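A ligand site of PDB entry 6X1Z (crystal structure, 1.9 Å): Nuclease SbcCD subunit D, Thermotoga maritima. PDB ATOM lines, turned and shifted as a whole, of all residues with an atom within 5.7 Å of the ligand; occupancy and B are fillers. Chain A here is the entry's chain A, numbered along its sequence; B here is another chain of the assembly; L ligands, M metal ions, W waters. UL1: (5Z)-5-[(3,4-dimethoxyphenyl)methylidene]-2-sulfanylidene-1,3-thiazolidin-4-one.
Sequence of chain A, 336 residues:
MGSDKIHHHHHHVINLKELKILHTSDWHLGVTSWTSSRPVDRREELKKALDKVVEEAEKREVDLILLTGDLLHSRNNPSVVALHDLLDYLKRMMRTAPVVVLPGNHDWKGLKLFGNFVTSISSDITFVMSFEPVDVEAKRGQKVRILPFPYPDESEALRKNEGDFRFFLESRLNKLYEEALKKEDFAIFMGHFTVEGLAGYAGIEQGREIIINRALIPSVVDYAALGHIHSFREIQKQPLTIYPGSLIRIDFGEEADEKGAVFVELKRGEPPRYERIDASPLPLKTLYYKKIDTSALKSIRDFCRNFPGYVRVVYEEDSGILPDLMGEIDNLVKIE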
ATOM      1  N   GLY A  69      12.365  -3.508 -22.674  1.00  0.00           N
ATOM      2  CA  GLY A  69      11.234  -2.997 -23.444  1.00  0.00           C
ATOM      3  C   GLY A  69      11.608  -1.927 -24.446  1.00  0.00           C
ATOM      4  O   GLY A  69      12.744  -1.445 -24.523  1.00  0.00           O
ATOM      5  N   ASP A  70      10.604  -1.520 -25.225  1.00  0.00           N
ATOM      6  CA  ASP A  70      10.819  -0.660 -26.397  1.00  0.00           C
ATOM      7  C   ASP A  70      11.871  -1.271 -27.316  1.00  0.00           C
ATOM      8  O   ASP A  70      12.719  -0.588 -27.875  1.00  0.00           O
ATOM      9  CB  ASP A  70      11.220   0.764 -25.989  1.00  0.00           C
ATOM     10  CG  ASP A  70      10.045   1.607 -25.501  1.00  0.00           C
ATOM     11  OD1 ASP A  70       8.895   1.311 -25.889  1.00  0.00           O
ATOM     12  OD2 ASP A  70      10.266   2.540 -24.703  1.00  0.00           O
ATOM     13  N   LEU A  71      11.825  -2.591 -27.449  1.00  0.00           N
ATOM     14  CA  LEU A  71      12.705  -3.274 -28.385  1.00  0.00           C
ATOM     15  C   LEU A  71      12.291  -3.036 -29.827  1.00  0.00           C
ATOM     16  O   LEU A  71      13.086  -3.278 -30.735  1.00  0.00           O
ATOM     17  CB  LEU A  71      12.723  -4.772 -28.082  1.00  0.00           C
ATOM     18  CG  LEU A  71      13.060  -5.215 -26.648  1.00  0.00           C
ATOM     19  CD1 LEU A  71      13.161  -6.756 -26.545  1.00  0.00           C
ATOM     20  CD2 LEU A  71      14.359  -4.533 -26.138  1.00  0.00           C
ATOM     21  N   LEU A  72      11.067  -2.592 -30.054  1.00  0.00           N
ATOM     22  CA  LEU A  72      10.600  -2.243 -31.384  1.00  0.00           C
ATOM     23  C   LEU A  72      10.226  -0.776 -31.398  1.00  0.00           C
ATOM     24  O   LEU A  72       9.653  -0.291 -30.440  1.00  0.00           O
ATOM     25  CB  LEU A  72       9.360  -3.070 -31.792  1.00  0.00           C
ATOM     26  CG  LEU A  72       9.611  -4.566 -31.970  1.00  0.00           C
ATOM     27  CD1 LEU A  72       8.284  -5.265 -31.962  1.00  0.00           C
ATOM     28  CD2 LEU A  72      10.363  -4.865 -33.266  1.00  0.00           C
ATOM     29  N   ASN A  76       2.642   0.163 -33.170  1.00  0.00           N
ATOM     30  CA  ASN A  76       1.718  -0.546 -34.044  1.00  0.00           C
ATOM     31  C   ASN A  76       2.396  -1.787 -34.601  1.00  0.00           C
ATOM     32  O   ASN A  76       3.457  -2.208 -34.130  1.00  0.00           O
ATOM     33  CB  ASN A  76       1.240   0.356 -35.186  1.00  0.00           C
ATOM     34  CG  ASN A  76       0.969   1.765 -34.732  1.00  0.00           C
ATOM     35  OD1 ASN A  76       1.705   2.693 -35.065  1.00  0.00           O
ATOM     36  ND2 ASN A  76      -0.110   1.941 -33.964  1.00  0.00           N
ATOM     37  N   PRO A  78       4.830  -3.848 -36.261  1.00  0.00           N
ATOM     38  CA  PRO A  78       6.161  -3.602 -36.814  1.00  0.00           C
ATOM     39  C   PRO A  78       6.279  -4.243 -38.191  1.00  0.00           C
ATOM     40  O   PRO A  78       5.549  -5.169 -38.557  1.00  0.00           O
ATOM     41  CB  PRO A  78       7.079  -4.278 -35.814  1.00  0.00           C
ATOM     42  CG  PRO A  78       6.247  -5.413 -35.284  1.00  0.00           C
ATOM     43  CD  PRO A  78       4.848  -4.877 -35.204  1.00  0.00           C
ATOM     44  N   LEU A  83      10.414  -7.316 -37.020  1.00  0.00           N
ATOM     45  CA  LEU A  83      10.084  -8.491 -36.224  1.00  0.00           C
ATOM     46  C   LEU A  83      11.091  -9.603 -36.455  1.00  0.00           C
ATOM     47  O   LEU A  83      11.503 -10.294 -35.505  1.00  0.00           O
ATOM     48  CB  LEU A  83       8.669  -8.947 -36.559  1.00  0.00           C
ATOM     49  CG  LEU A  83       8.204 -10.165 -35.755  1.00  0.00           C
ATOM     50  CD1 LEU A  83       8.305  -9.908 -34.275  1.00  0.00           C
ATOM     51  CD2 LEU A  83       6.791 -10.554 -36.144  1.00  0.00           C
ATOM     52  N   LEU A  86      14.080  -8.746 -34.385  1.00  0.00           N
ATOM     53  CA  LEU A  86      13.851  -8.887 -32.956  1.00  0.00           C
ATOM     54  C   LEU A  86      13.957 -10.348 -32.542  1.00  0.00           C
ATOM     55  O   LEU A  86      14.680 -10.702 -31.617  1.00  0.00           O
ATOM     56  CB  LEU A  86      12.476  -8.320 -32.599  1.00  0.00           C
ATOM     57  CG  LEU A  86      12.003  -8.637 -31.172  1.00  0.00           C
ATOM     58  CD1 LEU A  86      12.908  -7.987 -30.142  1.00  0.00           C
ATOM     59  CD2 LEU A  86      10.588  -8.158 -30.980  1.00  0.00           C
ATOM     60  N   LEU A  87      13.254 -11.214 -33.262  1.00  0.00           N
ATOM     61  CA  LEU A  87      13.291 -12.655 -32.981  1.00  0.00           C
ATOM     62  C   LEU A  87      14.654 -13.251 -33.232  1.00  0.00           C
ATOM     63  O   LEU A  87      15.066 -14.148 -32.506  1.00  0.00           O
ATOM     64  CB  LEU A  87      12.248 -13.394 -33.845  1.00  0.00           C
ATOM     65  CG  LEU A  87      10.776 -13.046 -33.566  1.00  0.00           C
ATOM     66  CD1 LEU A  87       9.801 -13.733 -34.499  1.00  0.00           C
ATOM     67  CD2 LEU A  87      10.418 -13.378 -32.124  1.00  0.00           C
ATOM     68  N   LEU A  90      16.697 -12.315 -30.258  1.00  0.00           N
ATOM     69  CA  LEU A  90      16.255 -13.089 -29.097  1.00  0.00           C
ATOM     70  C   LEU A  90      16.895 -14.461 -29.126  1.00  0.00           C
ATOM     71  O   LEU A  90      17.408 -14.951 -28.113  1.00  0.00           O
ATOM     72  CB  LEU A  90      14.732 -13.212 -29.066  1.00  0.00           C
ATOM     73  CG  LEU A  90      13.949 -11.968 -28.649  1.00  0.00           C
ATOM     74  CD1 LEU A  90      12.455 -12.267 -28.485  1.00  0.00           C
ATOM     75  CD2 LEU A  90      14.563 -11.347 -27.362  1.00  0.00           C
ATOM     76  N   VAL A 101      12.329 -11.126 -20.560  1.00  0.00           N
ATOM     77  CA  VAL A 101      11.854 -10.029 -21.407  1.00  0.00           C
ATOM     78  C   VAL A 101      10.691  -9.320 -20.716  1.00  0.00           C
ATOM     79  O   VAL A 101       9.638  -9.934 -20.500  1.00  0.00           O
ATOM     80  CB  VAL A 101      11.396 -10.529 -22.786  1.00  0.00           C
ATOM     81  CG1 VAL A 101      10.912  -9.358 -23.637  1.00  0.00           C
ATOM     82  CG2 VAL A 101      12.532 -11.302 -23.455  1.00  0.00           C
ATOM     83  N   LEU A 102      10.877  -8.032 -20.421  1.00  0.00           N
ATOM     84  CA  LEU A 102       9.786  -7.159 -19.968  1.00  0.00           C
ATOM     85  C   LEU A 102       9.498  -6.232 -21.125  1.00  0.00           C
ATOM     86  O   LEU A 102      10.247  -5.272 -21.330  1.00  0.00           O
ATOM     87  CB  LEU A 102      10.188  -6.359 -18.716  1.00  0.00           C
ATOM     88  CG  LEU A 102       9.128  -5.397 -18.156  1.00  0.00           C
ATOM     89  CD1 LEU A 102       8.172  -6.127 -17.188  1.00  0.00           C
ATOM     90  CD2 LEU A 102       9.816  -4.229 -17.448  1.00  0.00           C
ATOM     91  N   PRO A 103       8.476  -6.488 -21.935  1.00  0.00           N
ATOM     92  CA  PRO A 103       8.240  -5.622 -23.098  1.00  0.00           C
ATOM     93  C   PRO A 103       7.736  -4.244 -22.676  1.00  0.00           C
ATOM     94  O   PRO A 103       7.145  -4.079 -21.600  1.00  0.00           O
ATOM     95  CB  PRO A 103       7.198  -6.385 -23.909  1.00  0.00           C
ATOM     96  CG  PRO A 103       6.620  -7.403 -22.999  1.00  0.00           C
ATOM     97  CD  PRO A 103       7.670  -7.724 -21.975  1.00  0.00           C
ATOM     98  N   GLY A 104       7.924  -3.290 -23.587  1.00  0.00           N
ATOM     99  CA  GLY A 104       7.360  -1.962 -23.450  1.00  0.00           C
ATOM    100  C   GLY A 104       5.857  -1.962 -23.706  1.00  0.00           C
ATOM    101  O   GLY A 104       5.189  -2.988 -23.739  1.00  0.00           O
ATOM    102  N   ASN A 105       5.324  -0.753 -23.898  1.00  0.00           N
ATOM    103  CA  ASN A 105       3.875  -0.570 -24.014  1.00  0.00           C
ATOM    104  C   ASN A 105       3.424  -0.771 -25.464  1.00  0.00           C
ATOM    105  O   ASN A 105       2.851   0.105 -26.109  1.00  0.00           O
ATOM    106  CB  ASN A 105       3.479   0.808 -23.497  1.00  0.00           C
ATOM    107  CG  ASN A 105       1.982   1.055 -23.539  1.00  0.00           C
ATOM    108  OD1 ASN A 105       1.207   0.125 -23.320  1.00  0.00           O
ATOM    109  ND2 ASN A 105       1.571   2.286 -23.827  1.00  0.00           N
ATOM    110  N   HIS A 106       3.643  -1.983 -25.988  1.00  0.00           N
ATOM    111  CA  HIS A 106       3.250  -2.248 -27.363  1.00  0.00           C
ATOM    112  C   HIS A 106       1.742  -2.466 -27.463  1.00  0.00           C
ATOM    113  O   HIS A 106       1.088  -2.883 -26.504  1.00  0.00           O
ATOM    114  CB  HIS A 106       4.004  -3.473 -27.897  1.00  0.00           C
ATOM    115  CG  HIS A 106       4.090  -3.497 -29.393  1.00  0.00           C
ATOM    116  ND1 HIS A 106       3.117  -4.080 -30.180  1.00  0.00           N
ATOM    117  CD2 HIS A 106       5.002  -2.965 -30.236  1.00  0.00           C
ATOM    118  CE1 HIS A 106       3.437  -3.912 -31.450  1.00  0.00           C
ATOM    119  NE2 HIS A 106       4.578  -3.251 -31.515  1.00  0.00           N
ATOM    120  N   TRP A 108       0.125  -4.568 -29.687  1.00  0.00           N
ATOM    121  CA  TRP A 108      -0.311  -5.881 -30.144  1.00  0.00           C
ATOM    122  C   TRP A 108      -1.012  -6.639 -29.017  1.00  0.00           C
ATOM    123  O   TRP A 108      -0.403  -6.934 -27.986  1.00  0.00           O
ATOM    124  CB  TRP A 108       0.881  -6.698 -30.634  1.00  0.00           C
ATOM    125  CG  TRP A 108       0.427  -8.007 -31.199  1.00  0.00           C
ATOM    126  CD1 TRP A 108      -0.751  -8.269 -31.842  1.00  0.00           C
ATOM    127  CD2 TRP A 108       1.147  -9.248 -31.161  1.00  0.00           C
ATOM    128  NE1 TRP A 108      -0.808  -9.592 -32.221  1.00  0.00           N
ATOM    129  CE2 TRP A 108       0.352 -10.216 -31.816  1.00  0.00           C
ATOM    130  CE3 TRP A 108       2.395  -9.631 -30.656  1.00  0.00           C
ATOM    131  CZ2 TRP A 108       0.753 -11.552 -31.967  1.00  0.00           C
ATOM    132  CZ3 TRP A 108       2.800 -10.958 -30.797  1.00  0.00           C
ATOM    133  CH2 TRP A 108       1.985 -11.902 -31.456  1.00  0.00           C
ATOM    134  N   LEU A 111       0.407 -10.052 -27.809  1.00  0.00           N
ATOM    135  CA  LEU A 111       1.760 -10.143 -27.257  1.00  0.00           C
ATOM    136  C   LEU A 111       1.785 -10.973 -25.994  1.00  0.00           C
ATOM    137  O   LEU A 111       2.697 -11.777 -25.780  1.00  0.00           O
ATOM    138  CB  LEU A 111       2.349  -8.757 -26.967  1.00  0.00           C
ATOM    139  CG  LEU A 111       3.799  -8.772 -26.458  1.00  0.00           C
ATOM    140  CD1 LEU A 111       4.689  -9.592 -27.404  1.00  0.00           C
ATOM    141  CD2 LEU A 111       4.348  -7.351 -26.316  1.00  0.00           C
ATOM    142  N   PHE A 114       1.578 -14.730 -27.104  1.00  0.00           N
ATOM    143  CA  PHE A 114       2.882 -15.161 -27.608  1.00  0.00           C
ATOM    144  C   PHE A 114       3.873 -15.317 -26.468  1.00  0.00           C
ATOM    145  O   PHE A 114       4.557 -16.351 -26.365  1.00  0.00           O
ATOM    146  CB  PHE A 114       3.404 -14.141 -28.629  1.00  0.00           C
ATOM    147  CG  PHE A 114       4.850 -14.320 -29.015  1.00  0.00           C
ATOM    148  CD1 PHE A 114       5.861 -13.663 -28.315  1.00  0.00           C
ATOM    149  CD2 PHE A 114       5.211 -15.133 -30.081  1.00  0.00           C
ATOM    150  CE1 PHE A 114       7.214 -13.845 -28.657  1.00  0.00           C
ATOM    151  CE2 PHE A 114       6.548 -15.311 -30.441  1.00  0.00           C
ATOM    152  CZ  PHE A 114       7.560 -14.671 -29.725  1.00  0.00           C
ATOM    153  N   PHE A 127       8.901 -14.252 -20.560  1.00  0.00           N
ATOM    154  CA  PHE A 127       8.241 -12.968 -20.767  1.00  0.00           C
ATOM    155  C   PHE A 127       7.503 -12.622 -19.481  1.00  0.00           C
ATOM    156  O   PHE A 127       6.725 -13.443 -18.986  1.00  0.00           O
ATOM    157  CB  PHE A 127       7.246 -13.024 -21.930  1.00  0.00           C
ATOM    158  CG  PHE A 127       7.876 -12.765 -23.259  1.00  0.00           C
ATOM    159  CD1 PHE A 127       8.664 -13.726 -23.863  1.00  0.00           C
ATOM    160  CD2 PHE A 127       7.691 -11.558 -23.899  1.00  0.00           C
ATOM    161  CE1 PHE A 127       9.291 -13.477 -25.090  1.00  0.00           C
ATOM    162  CE2 PHE A 127       8.296 -11.298 -25.126  1.00  0.00           C
ATOM    163  CZ  PHE A 127       9.096 -12.273 -25.722  1.00  0.00           C
ATOM    164  N   TRP B 108      -1.495 -13.293 -41.905  1.00  0.00           N
ATOM    165  CA  TRP B 108      -0.476 -12.697 -41.038  1.00  0.00           C
ATOM    166  C   TRP B 108       0.926 -12.827 -41.634  1.00  0.00           C
ATOM    167  O   TRP B 108       1.448 -13.933 -41.791  1.00  0.00           O
ATOM    168  CB  TRP B 108      -0.539 -13.329 -39.637  1.00  0.00           C
ATOM    169  CG  TRP B 108       0.408 -12.672 -38.694  1.00  0.00           C
ATOM    170  CD1 TRP B 108       0.803 -11.359 -38.719  1.00  0.00           C
ATOM    171  CD2 TRP B 108       1.106 -13.283 -37.607  1.00  0.00           C
ATOM    172  NE1 TRP B 108       1.708 -11.129 -37.711  1.00  0.00           N
ATOM    173  CE2 TRP B 108       1.908 -12.285 -37.004  1.00  0.00           C
ATOM    174  CE3 TRP B 108       1.116 -14.581 -37.080  1.00  0.00           C
ATOM    175  CZ2 TRP B 108       2.713 -12.544 -35.889  1.00  0.00           C
ATOM    176  CZ3 TRP B 108       1.925 -14.843 -35.974  1.00  0.00           C
ATOM    177  CH2 TRP B 108       2.717 -13.829 -35.402  1.00  0.00           C
ATOM    178  N   PHE B 114       7.094 -16.289 -36.682  1.00  0.00           N
ATOM    179  CA  PHE B 114       6.662 -16.988 -35.475  1.00  0.00           C
ATOM    180  C   PHE B 114       6.980 -18.464 -35.590  1.00  0.00           C
ATOM    181  O   PHE B 114       7.592 -19.043 -34.690  1.00  0.00           O
ATOM    182  CB  PHE B 114       5.163 -16.773 -35.242  1.00  0.00           C
ATOM    183  CG  PHE B 114       4.574 -17.658 -34.167  1.00  0.00           C
ATOM    184  CD1 PHE B 114       4.600 -17.279 -32.831  1.00  0.00           C
ATOM    185  CD2 PHE B 114       3.959 -18.867 -34.501  1.00  0.00           C
ATOM    186  CE1 PHE B 114       4.063 -18.090 -31.838  1.00  0.00           C
ATOM    187  CE2 PHE B 114       3.422 -19.694 -33.513  1.00  0.00           C
ATOM    188  CZ  PHE B 114       3.459 -19.295 -32.180  1.00  0.00           C
HETATM  189  CAA UL1 L   1       6.050 -12.032 -31.633  1.00  0.00           C
HETATM  190  CAB UL1 L   1       5.217  -6.720 -31.513  1.00  0.00           C
HETATM  191  CAE UL1 L   1       8.620  -7.723 -27.786  1.00  0.00           C
HETATM  192  CAF UL1 L   1       8.246  -9.715 -29.029  1.00  0.00           C
HETATM  193  CAG UL1 L   1       7.621 -10.468 -30.034  1.00  0.00           C
HETATM  194  CAH UL1 L   1       6.907  -7.807 -29.607  1.00  0.00           C
HETATM  195  CAM UL1 L   1       7.886  -8.393 -28.792  1.00  0.00           C
HETATM  196  CAN UL1 L   1       6.646  -9.891 -30.823  1.00  0.00           C
HETATM  197  CAO UL1 L   1       6.252  -8.576 -30.574  1.00  0.00           C
HETATM  198  CAP UL1 L   1       9.378  -5.805 -26.368  1.00  0.00           C
HETATM  199  CAQ UL1 L   1       8.362  -3.946 -27.022  1.00  0.00           C
HETATM  200  CAR UL1 L   1       8.581  -6.381 -27.392  1.00  0.00           C
HETATM  201  NAI UL1 L   1       9.223  -4.475 -26.146  1.00  0.00           N
HETATM  202  OAC UL1 L   1      10.105  -6.482 -25.661  1.00  0.00           O
HETATM  203  OAJ UL1 L   1       6.007 -10.599 -31.803  1.00  0.00           O
HETATM  204  OAK UL1 L   1       5.272  -8.113 -31.407  1.00  0.00           O
HETATM  205  SAD UL1 L   1       7.863  -2.366 -27.130  1.00  0.00           S
HETATM  206  SAL UL1 L   1       7.749  -5.079 -28.091  1.00  0.00           S
HETATM  207 MG    MG M   1       7.013   1.822 -24.000  1.00  0.00          MG
HETATM  208  O   HOH W   1      11.854  -6.245 -23.653  1.00  0.00           O
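Water W1 lies within hydrogen-bond range of an oxygen (OAC) of the ligand (2.7 Å), the backbone NH of Gly 69 (3.0 Å) and the backbone carbonyl oxygen of Leu 102 (3.0 Å).
The backbone NH of Gly 104 lies close to a sulfur (SAD) of the ligand (3.7 Å). N of Asp 70 sits close to SAD of the ligand, 3.4 Å away.
A ring nitrogen (ND1) of His 106 sits at hydrogen-bond distance from the backbone NH of Trp 108 of chain A, at 3.1 Å. O of Asn 76 lies within hydrogen-bond range of NE2 of His 106 (3.0 Å). The backbone carbonyl oxygen (O) of Leu 102 sits at hydrogen-bond distance from the backbone NH (N) of Gly 69 (3.1 Å).
NAI of the ligand sits close to N of Leu 71 (3.5 Å). Residues that only touch the ligand: Pro 103 (3.3 Å), His 106 (3.3 Å), Trp 108 of chain A (3.3 Å), Leu 86 (3.4 Å), Leu 72 (3.4 Å), Leu 83 (3.4 Å), Phe 114 of chain A (3.5 Å), Leu 111 (3.6 Å), Val 101 (3.6 Å) and Gly 69 (3.7 Å). Hydrophobic or aromatic side chains within 4 Å of the ligand: Leu 71, Leu 72, Leu 83, Leu 86, Val 101, Pro 103, His 106, Trp 108 of chain A, Leu 111 and Phe 114 of chain A. Within 4 Å of the ligand: Gly 69, Asp 70, Leu 71, Leu 72, Leu 83, Leu 86, Val 101, Pro 103, Gly 104, His 106, Trp 108 of chain A, Leu 111 and Phe 114 of chain A.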
